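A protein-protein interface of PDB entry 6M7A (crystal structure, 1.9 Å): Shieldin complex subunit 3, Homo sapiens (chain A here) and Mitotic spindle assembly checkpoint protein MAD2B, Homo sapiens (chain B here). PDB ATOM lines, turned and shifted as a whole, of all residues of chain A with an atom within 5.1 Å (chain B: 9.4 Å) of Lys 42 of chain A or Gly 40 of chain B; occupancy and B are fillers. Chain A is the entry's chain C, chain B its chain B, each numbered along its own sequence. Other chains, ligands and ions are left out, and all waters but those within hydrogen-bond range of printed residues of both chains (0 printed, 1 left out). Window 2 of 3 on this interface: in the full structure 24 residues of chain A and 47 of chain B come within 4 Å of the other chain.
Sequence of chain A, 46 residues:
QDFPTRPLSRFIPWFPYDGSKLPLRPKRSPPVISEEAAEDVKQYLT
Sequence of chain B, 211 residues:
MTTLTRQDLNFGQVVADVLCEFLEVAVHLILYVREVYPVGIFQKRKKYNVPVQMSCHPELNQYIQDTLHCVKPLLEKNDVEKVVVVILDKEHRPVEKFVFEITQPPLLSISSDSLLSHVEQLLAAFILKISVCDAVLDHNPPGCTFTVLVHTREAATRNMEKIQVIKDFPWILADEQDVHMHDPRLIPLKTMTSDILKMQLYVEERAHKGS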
ATOM      1  N   ALA A  38       5.477 -23.369 -18.232  1.00  0.00           N
ATOM      2  CA  ALA A  38       5.812 -21.965 -18.011  1.00  0.00           C
ATOM      3  C   ALA A  38       7.322 -21.761 -17.912  1.00  0.00           C
ATOM      4  O   ALA A  38       7.854 -20.753 -18.394  1.00  0.00           O
ATOM      5  CB  ALA A  38       5.116 -21.460 -16.742  1.00  0.00           C
ATOM      6  N   GLU A  39       8.029 -22.704 -17.284  1.00  0.00           N
ATOM      7  CA  GLU A  39       9.479 -22.577 -17.141  1.00  0.00           C
ATOM      8  C   GLU A  39      10.182 -22.634 -18.491  1.00  0.00           C
ATOM      9  O   GLU A  39      11.105 -21.851 -18.754  1.00  0.00           O
ATOM     10  CB  GLU A  39      10.004 -23.670 -16.207  1.00  0.00           C
ATOM     11  CG  GLU A  39      11.447 -23.493 -15.767  1.00  0.00           C
ATOM     12  CD  GLU A  39      11.771 -22.070 -15.344  1.00  0.00           C
ATOM     13  OE1 GLU A  39      12.805 -21.534 -15.807  1.00  0.00           O
ATOM     14  OE2 GLU A  39      10.997 -21.487 -14.550  1.00  0.00           O
ATOM     15  N   ASP A  40       9.758 -23.548 -19.361  1.00  0.00           N
ATOM     16  CA  ASP A  40      10.334 -23.610 -20.699  1.00  0.00           C
ATOM     17  C   ASP A  40      10.083 -22.317 -21.475  1.00  0.00           C
ATOM     18  O   ASP A  40      10.987 -21.808 -22.148  1.00  0.00           O
ATOM     19  CB  ASP A  40       9.785 -24.824 -21.451  1.00  0.00           C
ATOM     20  CG  ASP A  40      10.102 -26.138 -20.745  1.00  0.00           C
ATOM     21  OD1 ASP A  40       9.427 -27.153 -21.025  1.00  0.00           O
ATOM     22  OD2 ASP A  40      11.031 -26.150 -19.905  1.00  0.00           O
ATOM     23  N   VAL A  41       8.860 -21.766 -21.399  1.00  0.00           N
ATOM     24  CA  VAL A  41       8.591 -20.486 -22.062  1.00  0.00           C
ATOM     25  C   VAL A  41       9.579 -19.431 -21.576  1.00  0.00           C
ATOM     26  O   VAL A  41      10.215 -18.732 -22.371  1.00  0.00           O
ATOM     27  CB  VAL A  41       7.135 -20.028 -21.832  1.00  0.00           C
ATOM     28  CG1 VAL A  41       6.922 -18.648 -22.445  1.00  0.00           C
ATOM     29  CG2 VAL A  41       6.132 -21.001 -22.430  1.00  0.00           C
ATOM     30  N   LYS A  42       9.715 -19.301 -20.256  1.00  0.00           N
ATOM     31  CA  LYS A  42      10.661 -18.348 -19.691  1.00  0.00           C
ATOM     32  C   LYS A  42      12.077 -18.592 -20.189  1.00  0.00           C
ATOM     33  O   LYS A  42      12.818 -17.641 -20.471  1.00  0.00           O
ATOM     34  CB  LYS A  42      10.631 -18.442 -18.172  1.00  0.00           C
ATOM     35  CG  LYS A  42      11.834 -17.820 -17.512  1.00  0.00           C
ATOM     36  CD  LYS A  42      11.815 -16.345 -17.822  1.00  0.00           C
ATOM     37  CE  LYS A  42      10.676 -15.619 -17.092  1.00  0.00           C
ATOM     38  NZ  LYS A  42      10.295 -14.304 -17.733  1.00  0.00           N
ATOM     39  N   GLN A  43      12.481 -19.859 -20.282  1.00  0.00           N
ATOM     40  CA  GLN A  43      13.865 -20.169 -20.628  1.00  0.00           C
ATOM     41  C   GLN A  43      14.171 -19.811 -22.077  1.00  0.00           C
ATOM     42  O   GLN A  43      15.201 -19.189 -22.370  1.00  0.00           O
ATOM     43  CB  GLN A  43      14.148 -21.650 -20.377  1.00  0.00           C
ATOM     44  CG  GLN A  43      14.417 -22.009 -18.925  1.00  0.00           C
ATOM     45  CD  GLN A  43      15.467 -21.121 -18.286  1.00  0.00           C
ATOM     46  OE1 GLN A  43      15.145 -20.104 -17.666  1.00  0.00           O
ATOM     47  NE2 GLN A  43      16.733 -21.503 -18.432  1.00  0.00           N
ATOM     48  N   TYR A  44      13.286 -20.192 -22.996  1.00  0.00           N
ATOM     49  CA  TYR A  44      13.573 -20.175 -24.425  1.00  0.00           C
ATOM     50  C   TYR A  44      12.913 -19.022 -25.172  1.00  0.00           C
ATOM     51  O   TYR A  44      13.517 -18.453 -26.087  1.00  0.00           O
ATOM     52  CB  TYR A  44      13.122 -21.496 -25.055  1.00  0.00           C
ATOM     53  CG  TYR A  44      13.870 -22.715 -24.555  1.00  0.00           C
ATOM     54  CD1 TYR A  44      13.202 -23.771 -23.944  1.00  0.00           C
ATOM     55  CD2 TYR A  44      15.243 -22.817 -24.708  1.00  0.00           C
ATOM     56  CE1 TYR A  44      13.891 -24.893 -23.496  1.00  0.00           C
ATOM     57  CE2 TYR A  44      15.932 -23.926 -24.261  1.00  0.00           C
ATOM     58  CZ  TYR A  44      15.259 -24.962 -23.662  1.00  0.00           C
ATOM     59  OH  TYR A  44      15.972 -26.056 -23.230  1.00  0.00           O
ATOM     60  N   LEU A  45      11.680 -18.667 -24.821  1.00  0.00           N
ATOM     61  CA  LEU A  45      10.883 -17.784 -25.655  1.00  0.00           C
ATOM     62  C   LEU A  45      10.895 -16.328 -25.203  1.00  0.00           C
ATOM     63  O   LEU A  45      10.424 -15.465 -25.951  1.00  0.00           O
ATOM     64  CB  LEU A  45       9.439 -18.301 -25.714  1.00  0.00           C
ATOM     65  CG  LEU A  45       9.376 -19.760 -26.182  1.00  0.00           C
ATOM     66  CD1 LEU A  45       7.952 -20.235 -26.421  1.00  0.00           C
ATOM     67  CD2 LEU A  45      10.221 -19.959 -27.440  1.00  0.00           C
ATOM     68  N   THR A  46      11.413 -16.029 -24.015  1.00  0.00           N
ATOM     69  CA  THR A  46      11.479 -14.648 -23.546  1.00  0.00           C
ATOM     70  C   THR A  46      12.932 -14.205 -23.416  1.00  0.00           C
ATOM     71  O   THR A  46      13.544 -13.750 -24.380  1.00  0.00           O
ATOM     72  CB  THR A  46      10.779 -14.460 -22.186  1.00  0.00           C
ATOM     73  OG1 THR A  46      11.665 -14.880 -21.146  1.00  0.00           O
ATOM     74  CG2 THR A  46       9.489 -15.275 -22.107  1.00  0.00           C
ATOM     75  N   LEU B  31      -4.166 -10.810 -17.815  1.00  0.00           N
ATOM     76  CA  LEU B  31      -3.656 -12.120 -17.406  1.00  0.00           C
ATOM     77  C   LEU B  31      -2.384 -11.980 -16.566  1.00  0.00           C
ATOM     78  O   LEU B  31      -2.189 -12.702 -15.575  1.00  0.00           O
ATOM     79  CB  LEU B  31      -3.395 -12.977 -18.653  1.00  0.00           C
ATOM     80  CG  LEU B  31      -4.631 -13.248 -19.519  1.00  0.00           C
ATOM     81  CD1 LEU B  31      -4.239 -14.069 -20.754  1.00  0.00           C
ATOM     82  CD2 LEU B  31      -5.732 -13.940 -18.703  1.00  0.00           C
ATOM     83  N   TYR B  32      -1.512 -11.048 -16.951  1.00  0.00           N
ATOM     84  CA  TYR B  32      -0.270 -10.829 -16.214  1.00  0.00           C
ATOM     85  C   TYR B  32      -0.540 -10.231 -14.840  1.00  0.00           C
ATOM     86  O   TYR B  32      -0.035 -10.712 -13.821  1.00  0.00           O
ATOM     87  CB  TYR B  32       0.638  -9.901 -17.017  1.00  0.00           C
ATOM     88  CG  TYR B  32       1.885  -9.441 -16.270  1.00  0.00           C
ATOM     89  CD1 TYR B  32       3.030 -10.218 -16.262  1.00  0.00           C
ATOM     90  CD2 TYR B  32       1.911  -8.226 -15.591  1.00  0.00           C
ATOM     91  CE1 TYR B  32       4.191  -9.802 -15.583  1.00  0.00           C
ATOM     92  CE2 TYR B  32       3.069  -7.801 -14.896  1.00  0.00           C
ATOM     93  CZ  TYR B  32       4.197  -8.595 -14.911  1.00  0.00           C
ATOM     94  OH  TYR B  32       5.345  -8.190 -14.250  1.00  0.00           O
ATOM     95  N   GLU B  35      -2.267 -12.452 -12.480  1.00  0.00           N
ATOM     96  CA  GLU B  35      -1.575 -13.727 -12.291  1.00  0.00           C
ATOM     97  C   GLU B  35      -2.458 -14.925 -12.650  1.00  0.00           C
ATOM     98  O   GLU B  35      -2.474 -15.934 -11.939  1.00  0.00           O
ATOM     99  CB  GLU B  35      -1.044 -13.839 -10.858  1.00  0.00           C
ATOM    100  CG  GLU B  35      -0.163 -12.653 -10.411  1.00  0.00           C
ATOM    101  CD  GLU B  35       0.361 -12.805  -8.978  1.00  0.00           C
ATOM    102  OE1 GLU B  35       1.410 -13.447  -8.785  1.00  0.00           O
ATOM    103  OE2 GLU B  35      -0.274 -12.283  -8.041  1.00  0.00           O
ATOM    104  N   TYR B  37      -1.857 -16.601 -15.290  1.00  0.00           N
ATOM    105  CA  TYR B  37      -0.748 -17.468 -15.661  1.00  0.00           C
ATOM    106  C   TYR B  37       0.511 -16.942 -14.980  1.00  0.00           C
ATOM    107  O   TYR B  37       0.566 -15.769 -14.590  1.00  0.00           O
ATOM    108  CB  TYR B  37      -0.547 -17.501 -17.189  1.00  0.00           C
ATOM    109  CG  TYR B  37      -1.713 -18.084 -17.977  1.00  0.00           C
ATOM    110  CD1 TYR B  37      -1.841 -19.455 -18.162  1.00  0.00           C
ATOM    111  CD2 TYR B  37      -2.673 -17.259 -18.548  1.00  0.00           C
ATOM    112  CE1 TYR B  37      -2.909 -19.994 -18.878  1.00  0.00           C
ATOM    113  CE2 TYR B  37      -3.754 -17.796 -19.278  1.00  0.00           C
ATOM    114  CZ  TYR B  37      -3.853 -19.158 -19.444  1.00  0.00           C
ATOM    115  OH  TYR B  37      -4.917 -19.686 -20.156  1.00  0.00           O
ATOM    116  N   PRO B  38       1.540 -17.780 -14.820  1.00  0.00           N
ATOM    117  CA  PRO B  38       2.750 -17.329 -14.115  1.00  0.00           C
ATOM    118  C   PRO B  38       3.439 -16.178 -14.833  1.00  0.00           C
ATOM    119  O   PRO B  38       3.490 -16.127 -16.065  1.00  0.00           O
ATOM    120  CB  PRO B  38       3.637 -18.575 -14.096  1.00  0.00           C
ATOM    121  CG  PRO B  38       2.717 -19.711 -14.280  1.00  0.00           C
ATOM    122  CD  PRO B  38       1.535 -19.236 -15.049  1.00  0.00           C
ATOM    123  N   VAL B  39       3.984 -15.257 -14.031  1.00  0.00           N
ATOM    124  CA  VAL B  39       4.719 -14.091 -14.529  1.00  0.00           C
ATOM    125  C   VAL B  39       5.765 -14.489 -15.564  1.00  0.00           C
ATOM    126  O   VAL B  39       6.054 -13.730 -16.504  1.00  0.00           O
ATOM    127  CB  VAL B  39       5.352 -13.338 -13.332  1.00  0.00           C
ATOM    128  CG1 VAL B  39       6.158 -14.282 -12.460  1.00  0.00           C
ATOM    129  CG2 VAL B  39       6.233 -12.207 -13.794  1.00  0.00           C
ATOM    130  N   GLY B  40       6.304 -15.703 -15.443  1.00  0.00           N
ATOM    131  CA  GLY B  40       7.410 -16.154 -16.264  1.00  0.00           C
ATOM    132  C   GLY B  40       7.103 -16.316 -17.740  1.00  0.00           C
ATOM    133  O   GLY B  40       8.029 -16.267 -18.559  1.00  0.00           O
ATOM    134  N   ILE B  41       5.835 -16.527 -18.110  1.00  0.00           N
ATOM    135  CA  ILE B  41       5.544 -16.675 -19.534  1.00  0.00           C
ATOM    136  C   ILE B  41       5.439 -15.339 -20.253  1.00  0.00           C
ATOM    137  O   ILE B  41       5.249 -15.325 -21.477  1.00  0.00           O
ATOM    138  CB  ILE B  41       4.251 -17.474 -19.804  1.00  0.00           C
ATOM    139  CG1 ILE B  41       3.016 -16.652 -19.426  1.00  0.00           C
ATOM    140  CG2 ILE B  41       4.283 -18.822 -19.099  1.00  0.00           C
ATOM    141  CD1 ILE B  41       1.721 -17.115 -20.114  1.00  0.00           C
ATOM    142  N   PHE B  42       5.570 -14.218 -19.547  1.00  0.00           N
ATOM    143  CA  PHE B  42       5.327 -12.909 -20.136  1.00  0.00           C
ATOM    144  C   PHE B  42       6.631 -12.204 -20.468  1.00  0.00           C
ATOM    145  O   PHE B  42       7.627 -12.363 -19.764  1.00  0.00           O
ATOM    146  CB  PHE B  42       4.502 -12.037 -19.190  1.00  0.00           C
ATOM    147  CG  PHE B  42       3.105 -12.523 -19.013  1.00  0.00           C
ATOM    148  CD1 PHE B  42       2.105 -12.115 -19.878  1.00  0.00           C
ATOM    149  CD2 PHE B  42       2.803 -13.425 -18.012  1.00  0.00           C
ATOM    150  CE1 PHE B  42       0.792 -12.581 -19.721  1.00  0.00           C
ATOM    151  CE2 PHE B  42       1.516 -13.883 -17.834  1.00  0.00           C
ATOM    152  CZ  PHE B  42       0.502 -13.468 -18.694  1.00  0.00           C
ATOM    153  N   GLN B  43       6.609 -11.413 -21.540  1.00  0.00           N
ATOM    154  CA  GLN B  43       7.737 -10.586 -21.953  1.00  0.00           C
ATOM    155  C   GLN B  43       7.303  -9.127 -22.012  1.00  0.00           C
ATOM    156  O   GLN B  43       6.210  -8.825 -22.493  1.00  0.00           O
ATOM    157  CB  GLN B  43       8.268 -11.042 -23.312  1.00  0.00           C
ATOM    158  CG  GLN B  43       9.345 -10.153 -23.916  1.00  0.00           C
ATOM    159  CD  GLN B  43       9.616 -10.501 -25.377  1.00  0.00           C
ATOM    160  OE1 GLN B  43      10.674 -11.021 -25.713  1.00  0.00           O
ATOM    161  NE2 GLN B  43       8.663 -10.213 -26.242  1.00  0.00           N
ATOM    162  N   LYS B  44       8.145  -8.227 -21.509  1.00  0.00           N
ATOM    163  CA  LYS B  44       7.794  -6.811 -21.516  1.00  0.00           C
ATOM    164  C   LYS B  44       7.911  -6.234 -22.922  1.00  0.00           C
ATOM    165  O   LYS B  44       8.865  -6.514 -23.656  1.00  0.00           O
ATOM    166  CB  LYS B  44       8.682  -6.010 -20.553  1.00  0.00           C
ATOM    167  CG  LYS B  44       8.227  -4.547 -20.402  1.00  0.00           C
ATOM    168  CD  LYS B  44       8.910  -3.825 -19.254  1.00  0.00           C
ATOM    169  CE  LYS B  44      10.342  -3.458 -19.607  1.00  0.00           C
ATOM    170  NZ  LYS B  44      11.311  -4.576 -19.390  1.00  0.00           N
ATOM    171  N   GLN B  53       2.992  -6.132 -20.965  1.00  0.00           N
ATOM    172  CA  GLN B  53       3.509  -7.492 -20.845  1.00  0.00           C
ATOM    173  C   GLN B  53       2.701  -8.411 -21.750  1.00  0.00           C
ATOM    174  O   GLN B  53       1.476  -8.471 -21.624  1.00  0.00           O
ATOM    175  CB  GLN B  53       3.436  -7.967 -19.392  1.00  0.00           C
ATOM    176  CG  GLN B  53       4.229  -7.109 -18.432  1.00  0.00           C
ATOM    177  CD  GLN B  53       5.675  -7.550 -18.348  1.00  0.00           C
ATOM    178  OE1 GLN B  53       6.526  -6.843 -17.765  1.00  0.00           O
ATOM    179  NE2 GLN B  53       5.973  -8.701 -18.929  1.00  0.00           N
ATOM    180  N   MET B  54       3.368  -9.114 -22.666  1.00  0.00           N
ATOM    181  CA  MET B  54       2.700 -10.072 -23.544  1.00  0.00           C
ATOM    182  C   MET B  54       3.193 -11.485 -23.293  1.00  0.00           C
ATOM    183  O   MET B  54       4.389 -11.704 -23.064  1.00  0.00           O
ATOM    184  CB  MET B  54       2.889  -9.730 -25.020  1.00  0.00           C
ATOM    185  CG  MET B  54       2.817  -8.259 -25.317  1.00  0.00           C
ATOM    186  SD  MET B  54       1.083  -7.754 -25.305  1.00  0.00           S
ATOM    187  CE  MET B  54       0.311  -8.735 -26.553  1.00  0.00           C
ATOM    188  N   SER B  55       2.257 -12.435 -23.354  1.00  0.00           N
ATOM    189  CA  SER B  55       2.595 -13.846 -23.248  1.00  0.00           C
ATOM    190  C   SER B  55       3.424 -14.302 -24.445  1.00  0.00           C
ATOM    191  O   SER B  55       3.161 -13.921 -25.596  1.00  0.00           O
ATOM    192  CB  SER B  55       1.306 -14.684 -23.151  1.00  0.00           C
ATOM    193  OG  SER B  55       1.530 -16.027 -23.567  1.00  0.00           O
ATOM    194  N   CYS B  56       4.422 -15.146 -24.171  1.00  0.00           N
ATOM    195  CA  CYS B  56       5.210 -15.796 -25.212  1.00  0.00           C
ATOM    196  C   CYS B  56       4.823 -17.259 -25.399  1.00  0.00           C
ATOM    197  O   CYS B  56       5.465 -17.970 -26.180  1.00  0.00           O
ATOM    198  CB  CYS B  56       6.704 -15.666 -24.902  1.00  0.00           C
ATOM    199  SG  CYS B  56       7.288 -13.929 -24.944  1.00  0.00           S
ATOM    200  N   HIS B  57       3.764 -17.711 -24.737  1.00  0.00           N
ATOM    201  CA  HIS B  57       3.269 -19.071 -24.921  1.00  0.00           C
ATOM    202  C   HIS B  57       2.471 -19.164 -26.219  1.00  0.00           C
ATOM    203  O   HIS B  57       1.460 -18.469 -26.362  1.00  0.00           O
ATOM    204  CB  HIS B  57       2.393 -19.472 -23.748  1.00  0.00           C
ATOM    205  CG  HIS B  57       1.908 -20.887 -23.817  1.00  0.00           C
ATOM    206  ND1 HIS B  57       0.701 -21.224 -24.384  1.00  0.00           N
ATOM    207  CD2 HIS B  57       2.445 -22.043 -23.362  1.00  0.00           C
ATOM    208  CE1 HIS B  57       0.524 -22.531 -24.300  1.00  0.00           C
ATOM    209  NE2 HIS B  57       1.564 -23.052 -23.675  1.00  0.00           N
ATOM    210  N   PRO B  58       2.870 -20.010 -27.171  1.00  0.00           N
ATOM    211  CA  PRO B  58       2.259 -19.922 -28.515  1.00  0.00           C
ATOM    212  C   PRO B  58       0.789 -20.279 -28.550  1.00  0.00           C
ATOM    213  O   PRO B  58       0.018 -19.618 -29.256  1.00  0.00           O
ATOM    214  CB  PRO B  58       3.101 -20.906 -29.349  1.00  0.00           C
ATOM    215  CG  PRO B  58       4.388 -21.013 -28.598  1.00  0.00           C
ATOM    216  CD  PRO B  58       4.022 -20.924 -27.147  1.00  0.00           C
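Among the printed residues, pairs that only touch across the chains: Ala 38 of chain A with Pro 38 of chain B (3.9 Å), Ala 38 of chain A with Ile 41 of chain B (3.6 Å), Val 41 of chain A with Ile 41 of chain B (3.8 Å), Val 41 of chain A with Cys 56 of chain B (3.9 Å), Val 41 of chain A with His 57 of chain B (3.9 Å), Lys 42 of chain A with Phe 42 of chain B (3.9 Å), Thr 46 of chain A with Gly 40 of chain B (3.96 Å) and Thr 46 of chain A with Cys 56 of chain B (3.8 Å).
The backbone carbonyl oxygen (O) of Gly 40 of chain B sits close to the side-chain amino group (NZ) of Lys 42 of chain A, at 3.1 Å. SG of Cys 56 of chain B is in hydrogen-bond range of O of Leu 45 of chain A.
Of chain B, only Gly 40 (3.1 Å) and Phe 42 (3.9 Å) come within 4 Å of Lys 42 of chain A. Of chain A, only Lys 42 and Thr 46 come within 4 Å of Gly 40 of chain B. Of chain B, only Ile 41, Cys 56 and His 57 come within 4 Å of Val 41 of chain A. Printed residues of chain A within 4 Å of Ile 41 of chain B: Ala 38 (3.6 Å) and Val 41 (3.8 Å). Printed residues of chain A within 4 Å of Pro 38 of chain B: Ala 38 (3.9 Å). Of the printed residues of chain B, Thr 46 of chain A touches Gly 40 (3.96 Å) and Cys 56 (3.8 Å). Gln 43 of chain A touches none of the printed residues of chain B. The nearest residue of chain B that does not touch Lys 42 of chain A is Val 39 of chain B (4.5 Å). The nearest residue of chain A that does not touch Gly 40 of chain B is Ala 38 of chain A (4.5 Å). The nearest printed residue of chain A that does not touch Cys 56 of chain B is Lys 42 of chain A (6.6 Å).
Of the 9 printed residues of chain A, 5 touch a printed residue of chain B. Printed residues of chain A that touch a printed residue of chain B: Ala 38, Val 41, Lys 42, Leu 45 and Thr 46. Among the printed residues, 10 pairs touch across the chains.
The backbone carbonyl oxygen (O) of Ile 41 of chain B sits at hydrogen-bond distance from the backbone NH (N) of Cys 56 of chain B, 2.8 Å away. The backbone NH of His 57 of chain B sits at hydrogen-bond distance from the side-chain hydroxyl of Ser 55 of chain B (3.0 Å). O of Val 41 of chain A sits at hydrogen-bond distance from N of Thr 46 of chain A, at 3.4 Å. The backbone carbonyl oxygen (O) of Lys 42 of chain A sits at hydrogen-bond distance from the side-chain hydroxyl (OG1) of Thr 46 of chain A.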
